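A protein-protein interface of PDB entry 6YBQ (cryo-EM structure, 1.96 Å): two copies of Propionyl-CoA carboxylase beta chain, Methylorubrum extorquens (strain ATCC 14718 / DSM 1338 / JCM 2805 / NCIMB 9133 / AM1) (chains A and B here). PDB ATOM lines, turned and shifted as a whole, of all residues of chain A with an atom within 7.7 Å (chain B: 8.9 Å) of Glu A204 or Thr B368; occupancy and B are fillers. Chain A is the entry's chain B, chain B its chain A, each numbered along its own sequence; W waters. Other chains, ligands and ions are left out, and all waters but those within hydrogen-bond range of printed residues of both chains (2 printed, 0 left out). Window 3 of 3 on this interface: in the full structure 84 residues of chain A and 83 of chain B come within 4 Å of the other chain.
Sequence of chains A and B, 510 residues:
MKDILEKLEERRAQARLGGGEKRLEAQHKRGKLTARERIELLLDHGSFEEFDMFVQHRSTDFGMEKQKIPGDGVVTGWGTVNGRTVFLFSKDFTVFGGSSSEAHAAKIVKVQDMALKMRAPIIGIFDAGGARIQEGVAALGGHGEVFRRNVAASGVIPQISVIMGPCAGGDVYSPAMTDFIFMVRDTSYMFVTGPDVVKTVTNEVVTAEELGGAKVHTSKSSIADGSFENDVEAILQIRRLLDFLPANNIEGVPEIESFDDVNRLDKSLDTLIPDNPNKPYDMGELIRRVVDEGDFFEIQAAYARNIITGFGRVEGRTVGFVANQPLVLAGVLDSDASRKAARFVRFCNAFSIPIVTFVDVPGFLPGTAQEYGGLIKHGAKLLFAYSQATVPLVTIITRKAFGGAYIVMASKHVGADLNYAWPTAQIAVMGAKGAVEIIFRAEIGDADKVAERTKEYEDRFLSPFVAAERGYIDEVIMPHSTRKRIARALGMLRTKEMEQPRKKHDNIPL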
ATOM      1  N   THR A 193     -21.162 -30.470 -24.386  1.00  0.00           N
ATOM      2  CA  THR A 193     -21.230 -29.615 -23.208  1.00  0.00           C
ATOM      3  C   THR A 193     -22.623 -29.006 -23.110  1.00  0.00           C
ATOM      4  O   THR A 193     -23.214 -28.622 -24.122  1.00  0.00           O
ATOM      5  CB  THR A 193     -20.164 -28.507 -23.260  1.00  0.00           C
ATOM      6  OG1 THR A 193     -18.856 -29.090 -23.203  1.00  0.00           O
ATOM      7  CG2 THR A 193     -20.327 -27.557 -22.106  1.00  0.00           C
ATOM      8  N   GLY A 194     -23.138 -28.914 -21.885  1.00  0.00           N
ATOM      9  CA  GLY A 194     -24.529 -28.603 -21.651  1.00  0.00           C
ATOM     10  C   GLY A 194     -24.841 -27.137 -21.416  1.00  0.00           C
ATOM     11  O   GLY A 194     -23.954 -26.285 -21.327  1.00  0.00           O
ATOM     12  N   PRO A 195     -26.137 -26.827 -21.289  1.00  0.00           N
ATOM     13  CA  PRO A 195     -26.559 -25.416 -21.226  1.00  0.00           C
ATOM     14  C   PRO A 195     -25.957 -24.615 -20.083  1.00  0.00           C
ATOM     15  O   PRO A 195     -25.610 -23.448 -20.283  1.00  0.00           O
ATOM     16  CB  PRO A 195     -28.085 -25.522 -21.090  1.00  0.00           C
ATOM     17  CG  PRO A 195     -28.437 -26.837 -21.635  1.00  0.00           C
ATOM     18  CD  PRO A 195     -27.285 -27.744 -21.379  1.00  0.00           C
ATOM     19  N   ASP A 196     -25.855 -25.183 -18.881  1.00  0.00           N
ATOM     20  CA  ASP A 196     -25.382 -24.403 -17.738  1.00  0.00           C
ATOM     21  C   ASP A 196     -23.952 -23.911 -17.955  1.00  0.00           C
ATOM     22  O   ASP A 196     -23.645 -22.732 -17.733  1.00  0.00           O
ATOM     23  CB  ASP A 196     -25.484 -25.242 -16.465  1.00  0.00           C
ATOM     24  CG  ASP A 196     -26.890 -25.746 -16.212  1.00  0.00           C
ATOM     25  OD1 ASP A 196     -27.801 -24.912 -16.028  1.00  0.00           O
ATOM     26  OD2 ASP A 196     -27.087 -26.978 -16.200  1.00  0.00           O
ATOM     27  N   VAL A 197     -23.060 -24.805 -18.380  1.00  0.00           N
ATOM     28  CA  VAL A 197     -21.689 -24.403 -18.684  1.00  0.00           C
ATOM     29  C   VAL A 197     -21.671 -23.383 -19.815  1.00  0.00           C
ATOM     30  O   VAL A 197     -20.887 -22.422 -19.798  1.00  0.00           O
ATOM     31  CB  VAL A 197     -20.834 -25.636 -19.030  1.00  0.00           C
ATOM     32  CG1 VAL A 197     -19.457 -25.205 -19.480  1.00  0.00           C
ATOM     33  CG2 VAL A 197     -20.734 -26.571 -17.847  1.00  0.00           C
ATOM     34  N   VAL A 198     -22.517 -23.589 -20.824  1.00  0.00           N
ATOM     35  CA  VAL A 198     -22.580 -22.662 -21.949  1.00  0.00           C
ATOM     36  C   VAL A 198     -22.932 -21.264 -21.458  1.00  0.00           C
ATOM     37  O   VAL A 198     -22.366 -20.266 -21.915  1.00  0.00           O
ATOM     38  CB  VAL A 198     -23.584 -23.174 -23.000  1.00  0.00           C
ATOM     39  CG1 VAL A 198     -23.990 -22.068 -23.950  1.00  0.00           C
ATOM     40  CG2 VAL A 198     -23.009 -24.368 -23.767  1.00  0.00           C
ATOM     41  N   LYS A 199     -23.863 -21.173 -20.509  1.00  0.00           N
ATOM     42  CA  LYS A 199     -24.199 -19.888 -19.906  1.00  0.00           C
ATOM     43  C   LYS A 199     -23.003 -19.310 -19.163  1.00  0.00           C
ATOM     44  O   LYS A 199     -22.622 -18.154 -19.375  1.00  0.00           O
ATOM     45  CB  LYS A 199     -25.393 -20.052 -18.961  1.00  0.00           C
ATOM     46  CG  LYS A 199     -25.729 -18.825 -18.115  1.00  0.00           C
ATOM     47  CD  LYS A 199     -26.345 -17.721 -18.943  1.00  0.00           C
ATOM     48  CE  LYS A 199     -26.888 -16.603 -18.066  1.00  0.00           C
ATOM     49  NZ  LYS A 199     -27.856 -17.099 -17.052  1.00  0.00           N
ATOM     50  N   THR A 200     -22.401 -20.107 -18.282  1.00  0.00           N
ATOM     51  CA  THR A 200     -21.303 -19.600 -17.465  1.00  0.00           C
ATOM     52  C   THR A 200     -20.159 -19.059 -18.312  1.00  0.00           C
ATOM     53  O   THR A 200     -19.507 -18.087 -17.917  1.00  0.00           O
ATOM     54  CB  THR A 200     -20.784 -20.695 -16.535  1.00  0.00           C
ATOM     55  OG1 THR A 200     -20.396 -21.838 -17.304  1.00  0.00           O
ATOM     56  CG2 THR A 200     -21.848 -21.095 -15.535  1.00  0.00           C
ATOM     57  N   VAL A 201     -19.900 -19.659 -19.469  1.00  0.00           N
ATOM     58  CA  VAL A 201     -18.712 -19.337 -20.253  1.00  0.00           C
ATOM     59  C   VAL A 201     -19.004 -18.318 -21.348  1.00  0.00           C
ATOM     60  O   VAL A 201     -18.198 -17.418 -21.584  1.00  0.00           O
ATOM     61  CB  VAL A 201     -18.100 -20.624 -20.844  1.00  0.00           C
ATOM     62  CG1 VAL A 201     -16.904 -20.285 -21.712  1.00  0.00           C
ATOM     63  CG2 VAL A 201     -17.688 -21.569 -19.735  1.00  0.00           C
ATOM     64  N   THR A 202     -20.141 -18.434 -22.030  1.00  0.00           N
ATOM     65  CA  THR A 202     -20.433 -17.607 -23.190  1.00  0.00           C
ATOM     66  C   THR A 202     -21.546 -16.595 -22.959  1.00  0.00           C
ATOM     67  O   THR A 202     -21.772 -15.747 -23.829  1.00  0.00           O
ATOM     68  CB  THR A 202     -20.813 -18.492 -24.387  1.00  0.00           C
ATOM     69  OG1 THR A 202     -22.077 -19.117 -24.142  1.00  0.00           O
ATOM     70  CG2 THR A 202     -19.759 -19.563 -24.621  1.00  0.00           C
ATOM     71  N   ASN A 203     -22.243 -16.658 -21.828  1.00  0.00           N
ATOM     72  CA  ASN A 203     -23.366 -15.788 -21.491  1.00  0.00           C
ATOM     73  C   ASN A 203     -24.588 -16.031 -22.365  1.00  0.00           C
ATOM     74  O   ASN A 203     -25.509 -15.206 -22.369  1.00  0.00           O
ATOM     75  CB  ASN A 203     -22.980 -14.307 -21.574  1.00  0.00           C
ATOM     76  CG  ASN A 203     -21.779 -13.970 -20.719  1.00  0.00           C
ATOM     77  OD1 ASN A 203     -20.744 -13.535 -21.223  1.00  0.00           O
ATOM     78  ND2 ASN A 203     -21.909 -14.168 -19.414  1.00  0.00           N
ATOM     79  N   GLU A 204     -24.632 -17.137 -23.103  1.00  0.00           N
ATOM     80  CA  GLU A 204     -25.742 -17.443 -23.991  1.00  0.00           C
ATOM     81  C   GLU A 204     -26.723 -18.366 -23.276  1.00  0.00           C
ATOM     82  O   GLU A 204     -26.313 -19.345 -22.645  1.00  0.00           O
ATOM     83  CB  GLU A 204     -25.233 -18.083 -25.286  1.00  0.00           C
ATOM     84  CG  GLU A 204     -26.292 -18.254 -26.351  1.00  0.00           C
ATOM     85  CD  GLU A 204     -25.733 -18.773 -27.665  1.00  0.00           C
ATOM     86  OE1 GLU A 204     -24.512 -19.027 -27.742  1.00  0.00           O
ATOM     87  OE2 GLU A 204     -26.517 -18.921 -28.625  1.00  0.00           O
ATOM     88  N   VAL A 205     -28.009 -18.037 -23.360  1.00  0.00           N
ATOM     89  CA  VAL A 205     -29.078 -18.828 -22.759  1.00  0.00           C
ATOM     90  C   VAL A 205     -29.686 -19.709 -23.844  1.00  0.00           C
ATOM     91  O   VAL A 205     -30.148 -19.207 -24.874  1.00  0.00           O
ATOM     92  CB  VAL A 205     -30.148 -17.931 -22.113  1.00  0.00           C
ATOM     93  CG1 VAL A 205     -31.257 -18.771 -21.499  1.00  0.00           C
ATOM     94  CG2 VAL A 205     -29.522 -17.035 -21.071  1.00  0.00           C
ATOM     95  N   VAL A 206     -29.687 -21.018 -23.608  1.00  0.00           N
ATOM     96  CA  VAL A 206     -30.209 -21.989 -24.565  1.00  0.00           C
ATOM     97  C   VAL A 206     -30.807 -23.165 -23.809  1.00  0.00           C
ATOM     98  O   VAL A 206     -30.321 -23.552 -22.743  1.00  0.00           O
ATOM     99  CB  VAL A 206     -29.116 -22.473 -25.543  1.00  0.00           C
ATOM    100  CG1 VAL A 206     -28.724 -21.374 -26.493  1.00  0.00           C
ATOM    101  CG2 VAL A 206     -27.904 -22.957 -24.777  1.00  0.00           C
ATOM    102  N   THR A 207     -31.867 -23.727 -24.374  1.00  0.00           N
ATOM    103  CA  THR A 207     -32.456 -24.972 -23.913  1.00  0.00           C
ATOM    104  C   THR A 207     -31.811 -26.155 -24.630  1.00  0.00           C
ATOM    105  O   THR A 207     -31.156 -26.006 -25.663  1.00  0.00           O
ATOM    106  CB  THR A 207     -33.966 -24.979 -24.156  1.00  0.00           C
ATOM    107  OG1 THR A 207     -34.221 -24.967 -25.563  1.00  0.00           O
ATOM    108  CG2 THR A 207     -34.634 -23.774 -23.504  1.00  0.00           C
ATOM    109  N   GLU A 210     -32.876 -26.479 -28.253  1.00  0.00           N
ATOM    110  CA  GLU A 210     -32.216 -25.499 -29.111  1.00  0.00           C
ATOM    111  C   GLU A 210     -30.745 -25.838 -29.316  1.00  0.00           C
ATOM    112  O   GLU A 210     -30.200 -25.623 -30.404  1.00  0.00           O
ATOM    113  CB  GLU A 210     -32.361 -24.098 -28.513  1.00  0.00           C
ATOM    114  CG  GLU A 210     -33.795 -23.617 -28.378  1.00  0.00           C
ATOM    115  CD  GLU A 210     -33.909 -22.280 -27.665  1.00  0.00           C
ATOM    116  OE1 GLU A 210     -34.682 -21.421 -28.137  1.00  0.00           O
ATOM    117  OE2 GLU A 210     -33.232 -22.086 -26.633  1.00  0.00           O
ATOM    118  N   LEU A 211     -30.087 -26.370 -28.286  1.00  0.00           N
ATOM    119  CA  LEU A 211     -28.654 -26.637 -28.366  1.00  0.00           C
ATOM    120  C   LEU A 211     -28.349 -27.890 -29.183  1.00  0.00           C
ATOM    121  O   LEU A 211     -27.440 -27.884 -30.018  1.00  0.00           O
ATOM    122  CB  LEU A 211     -28.064 -26.752 -26.955  1.00  0.00           C
ATOM    123  CG  LEU A 211     -26.549 -26.955 -26.827  1.00  0.00           C
ATOM    124  CD1 LEU A 211     -25.775 -25.860 -27.535  1.00  0.00           C
ATOM    125  CD2 LEU A 211     -26.118 -27.040 -25.370  1.00  0.00           C
ATOM    126  N   GLY A 212     -29.084 -28.980 -28.948  1.00  0.00           N
ATOM    127  CA  GLY A 212     -28.795 -30.248 -29.594  1.00  0.00           C
ATOM    128  C   GLY A 212     -29.971 -31.114 -30.015  1.00  0.00           C
ATOM    129  O   GLY A 212     -29.827 -32.334 -30.102  1.00  0.00           O
ATOM    130  N   VAL A 216     -31.680 -29.571 -35.211  1.00  0.00           N
ATOM    131  CA  VAL A 216     -30.300 -29.106 -35.320  1.00  0.00           C
ATOM    132  C   VAL A 216     -29.423 -30.157 -35.993  1.00  0.00           C
ATOM    133  O   VAL A 216     -28.711 -29.866 -36.959  1.00  0.00           O
ATOM    134  CB  VAL A 216     -29.762 -28.725 -33.927  1.00  0.00           C
ATOM    135  CG1 VAL A 216     -28.258 -28.627 -33.936  1.00  0.00           C
ATOM    136  CG2 VAL A 216     -30.354 -27.410 -33.458  1.00  0.00           C
ATOM    137  N   LYS A 220     -28.527 -29.057 -39.767  1.00  0.00           N
ATOM    138  CA  LYS A 220     -27.456 -28.071 -39.674  1.00  0.00           C
ATOM    139  C   LYS A 220     -26.076 -28.674 -39.453  1.00  0.00           C
ATOM    140  O   LYS A 220     -25.128 -28.290 -40.143  1.00  0.00           O
ATOM    141  CB  LYS A 220     -27.775 -27.077 -38.546  1.00  0.00           C
ATOM    142  CG  LYS A 220     -28.950 -26.170 -38.838  1.00  0.00           C
ATOM    143  CD  LYS A 220     -29.581 -25.637 -37.562  1.00  0.00           C
ATOM    144  CE  LYS A 220     -28.639 -24.723 -36.801  1.00  0.00           C
ATOM    145  NZ  LYS A 220     -28.531 -23.390 -37.441  1.00  0.00           N
ATOM    146  N   LEU B 365     -14.268 -27.005 -25.891  1.00  0.00           N
ATOM    147  CA  LEU B 365     -14.736 -25.624 -26.008  1.00  0.00           C
ATOM    148  C   LEU B 365     -16.262 -25.593 -26.080  1.00  0.00           C
ATOM    149  O   LEU B 365     -16.837 -26.208 -26.984  1.00  0.00           O
ATOM    150  CB  LEU B 365     -14.139 -24.959 -27.247  1.00  0.00           C
ATOM    151  CG  LEU B 365     -14.468 -23.480 -27.484  1.00  0.00           C
ATOM    152  CD1 LEU B 365     -13.892 -22.593 -26.400  1.00  0.00           C
ATOM    153  CD2 LEU B 365     -13.980 -23.026 -28.847  1.00  0.00           C
ATOM    154  N   PRO B 366     -16.948 -24.903 -25.169  1.00  0.00           N
ATOM    155  CA  PRO B 366     -18.413 -24.881 -25.195  1.00  0.00           C
ATOM    156  C   PRO B 366     -18.985 -23.809 -26.115  1.00  0.00           C
ATOM    157  O   PRO B 366     -18.336 -22.819 -26.453  1.00  0.00           O
ATOM    158  CB  PRO B 366     -18.789 -24.583 -23.737  1.00  0.00           C
ATOM    159  CG  PRO B 366     -17.593 -24.022 -23.105  1.00  0.00           C
ATOM    160  CD  PRO B 366     -16.406 -24.228 -23.979  1.00  0.00           C
ATOM    161  N   GLY B 367     -20.238 -24.033 -26.509  1.00  0.00           N
ATOM    162  CA  GLY B 367     -21.010 -23.038 -27.229  1.00  0.00           C
ATOM    163  C   GLY B 367     -21.769 -23.553 -28.437  1.00  0.00           C
ATOM    164  O   GLY B 367     -21.420 -24.584 -29.018  1.00  0.00           O
ATOM    165  N   THR B 368     -22.823 -22.828 -28.817  1.00  0.00           N
ATOM    166  CA  THR B 368     -23.591 -23.182 -30.005  1.00  0.00           C
ATOM    167  C   THR B 368     -22.713 -23.232 -31.248  1.00  0.00           C
ATOM    168  O   THR B 368     -22.935 -24.061 -32.135  1.00  0.00           O
ATOM    169  CB  THR B 368     -24.731 -22.188 -30.214  1.00  0.00           C
ATOM    170  OG1 THR B 368     -24.202 -20.861 -30.280  1.00  0.00           O
ATOM    171  CG2 THR B 368     -25.743 -22.285 -29.089  1.00  0.00           C
ATOM    172  N   ALA B 369     -21.740 -22.326 -31.352  1.00  0.00           N
ATOM    173  CA  ALA B 369     -20.848 -22.329 -32.507  1.00  0.00           C
ATOM    174  C   ALA B 369     -20.211 -23.699 -32.706  1.00  0.00           C
ATOM    175  O   ALA B 369     -20.206 -24.239 -33.816  1.00  0.00           O
ATOM    176  CB  ALA B 369     -19.770 -21.256 -32.349  1.00  0.00           C
ATOM    177  N   GLN B 370     -19.676 -24.279 -31.632  1.00  0.00           N
ATOM    178  CA  GLN B 370     -18.994 -25.562 -31.749  1.00  0.00           C
ATOM    179  C   GLN B 370     -19.975 -26.687 -32.069  1.00  0.00           C
ATOM    180  O   GLN B 370     -19.692 -27.536 -32.919  1.00  0.00           O
ATOM    181  CB  GLN B 370     -18.221 -25.862 -30.463  1.00  0.00           C
ATOM    182  CG  GLN B 370     -16.870 -25.177 -30.355  1.00  0.00           C
ATOM    183  CD  GLN B 370     -15.882 -25.651 -31.401  1.00  0.00           C
ATOM    184  OE1 GLN B 370     -15.497 -26.818 -31.427  1.00  0.00           O
ATOM    185  NE2 GLN B 370     -15.472 -24.746 -32.270  1.00  0.00           N
ATOM    186  N   GLU B 371     -21.132 -26.710 -31.405  1.00  0.00           N
ATOM    187  CA  GLU B 371     -22.087 -27.797 -31.616  1.00  0.00           C
ATOM    188  C   GLU B 371     -22.669 -27.756 -33.026  1.00  0.00           C
ATOM    189  O   GLU B 371     -22.704 -28.776 -33.721  1.00  0.00           O
ATOM    190  CB  GLU B 371     -23.209 -27.733 -30.578  1.00  0.00           C
ATOM    191  CG  GLU B 371     -22.779 -27.946 -29.135  1.00  0.00           C
ATOM    192  CD  GLU B 371     -22.085 -29.279 -28.892  1.00  0.00           C
ATOM    193  OE1 GLU B 371     -22.210 -30.191 -29.731  1.00  0.00           O
ATOM    194  OE2 GLU B 371     -21.418 -29.414 -27.845  1.00  0.00           O
ATOM    195  N   TYR B 372     -23.133 -26.583 -33.460  1.00  0.00           N
ATOM    196  CA  TYR B 372     -23.724 -26.440 -34.784  1.00  0.00           C
ATOM    197  C   TYR B 372     -22.716 -26.712 -35.893  1.00  0.00           C
ATOM    198  O   TYR B 372     -23.119 -27.058 -37.007  1.00  0.00           O
ATOM    199  CB  TYR B 372     -24.306 -25.032 -34.963  1.00  0.00           C
ATOM    200  CG  TYR B 372     -25.469 -24.668 -34.059  1.00  0.00           C
ATOM    201  CD1 TYR B 372     -26.090 -25.608 -33.250  1.00  0.00           C
ATOM    202  CD2 TYR B 372     -25.951 -23.368 -34.027  1.00  0.00           C
ATOM    203  CE1 TYR B 372     -27.147 -25.260 -32.437  1.00  0.00           C
ATOM    204  CE2 TYR B 372     -27.002 -23.015 -33.219  1.00  0.00           C
ATOM    205  CZ  TYR B 372     -27.599 -23.961 -32.427  1.00  0.00           C
ATOM    206  OH  TYR B 372     -28.650 -23.596 -31.623  1.00  0.00           O
ATOM    207  N   GLY B 373     -21.426 -26.552 -35.614  1.00  0.00           N
ATOM    208  CA  GLY B 373     -20.366 -26.871 -36.545  1.00  0.00           C
ATOM    209  C   GLY B 373     -19.890 -28.306 -36.546  1.00  0.00           C
ATOM    210  O   GLY B 373     -18.998 -28.639 -37.330  1.00  0.00           O
ATOM    211  N   GLY B 374     -20.439 -29.164 -35.689  1.00  0.00           N
ATOM    212  CA  GLY B 374     -20.149 -30.582 -35.750  1.00  0.00           C
ATOM    213  C   GLY B 374     -19.053 -31.089 -34.838  1.00  0.00           C
ATOM    214  O   GLY B 374     -18.374 -32.058 -35.192  1.00  0.00           O
ATOM    215  N   LEU B 375     -18.872 -30.481 -33.662  1.00  0.00           N
ATOM    216  CA  LEU B 375     -17.792 -30.885 -32.762  1.00  0.00           C
ATOM    217  C   LEU B 375     -17.841 -32.368 -32.414  1.00  0.00           C
ATOM    218  O   LEU B 375     -16.799 -32.973 -32.168  1.00  0.00           O
ATOM    219  CB  LEU B 375     -17.835 -30.049 -31.485  1.00  0.00           C
ATOM    220  CG  LEU B 375     -16.888 -30.459 -30.354  1.00  0.00           C
ATOM    221  CD1 LEU B 375     -15.440 -30.448 -30.820  1.00  0.00           C
ATOM    222  CD2 LEU B 375     -17.079 -29.562 -29.140  1.00  0.00           C
HETATM  223  O   HOH W   1     -21.725 -26.776 -25.783  1.00  0.00           O
HETATM  224  O   HOH W   2     -31.672 -24.687 -32.599  1.00  0.00           O
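OG1 of Thr B368 is in hydrogen-bond range of OE1 of Glu A204, 3.1 Å away.
OH of Tyr B372 sits at hydrogen-bond distance from O of Glu A210 (2.8 Å).
The backbone carbonyl oxygen (O) of Val A198 sits at hydrogen-bond distance from the side-chain hydroxyl (OG1) of Thr A202, 2.5 Å away.
The side-chain hydroxyl (OG1) of Thr A202 sits close to the backbone NH (N) of Glu A204, at 3.4 Å.
The backbone NH (N) of Thr A207 lies within hydrogen-bond range of the side-chain carboxylate (OE2) of Glu A210, 3.1 Å away.
Among the printed residues, merely in contact across the chains: Thr A193 with Pro B366 (3.7 Å), Thr A193 with Glu B371 (3.6 Å), Val A198 with Gly B367 (3.9 Å), Thr A202 with Pro B366 (3.998 Å), Leu A211 with Thr B368 (3.9 Å), Leu A211 with Glu B371 (3.99 Å), Leu A211 with Tyr B372 (3.6 Å), Val A216 with Tyr B372 (3.8 Å) and Lys A220 with Tyr B372 (3.9 Å).
Of chain B, only Thr B368 (3.1 Å) comes within 4 Å of Glu A204.
Thr B368 touches just these residues of chain A: Glu A204 and Leu A211.
Of the printed residues of chain A, Tyr B372 touches Glu A210 (2.8 Å), Leu A211 (3.6 Å), Val A216 (3.8 Å) and Lys A220 (3.9 Å).
Of the printed residues of chain A, Gly B367 touches Val A198.
Printed residues of chain B within 4 Å of Lys A220: Tyr B372 (3.9 Å).
Printed residues of chain B within 4 Å of Thr A202: Pro B366 (3.998 Å).
Of the printed residues of chain B, Thr A193 touches Pro B366 and Glu B371.
Leu B375 touches none of the printed residues of chain A.
The nearest residue of chain A that does not touch Thr B368 is Val A206 (4.1 Å).
The nearest printed residue of chain A that does not touch Pro B366 is Val A201 (4.05 Å).
Of the 20 printed residues of chain A, 8 touch a printed residue of chain B.
Of the 11 printed residues of chain B, 5 touch a printed residue of chain A.
Printed residues of chain B that touch a printed residue of chain A: Pro B366, Gly B367, Thr B368, Glu B371 and Tyr B372.
Among the printed residues, no Asp or Glu carboxylate lies within 4 Å of a Lys or Arg side-chain nitrogen of the other chain.
No position is printed for both chains.
Of the 11 pairs that touch across the chains among the printed residues, none has its exchanged pair printed and touching as well.
Water W2 lies within hydrogen-bond range of O of Glu A210 (2.8 Å) and OH of Tyr B372 (3.4 Å).
Water W1 lies within hydrogen-bond range of the backbone carbonyl oxygen of Thr A193 (2.9 Å), the backbone NH of Gly B367 (3.2 Å) and the side-chain carboxylate of Glu B371 (3.4 Å).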
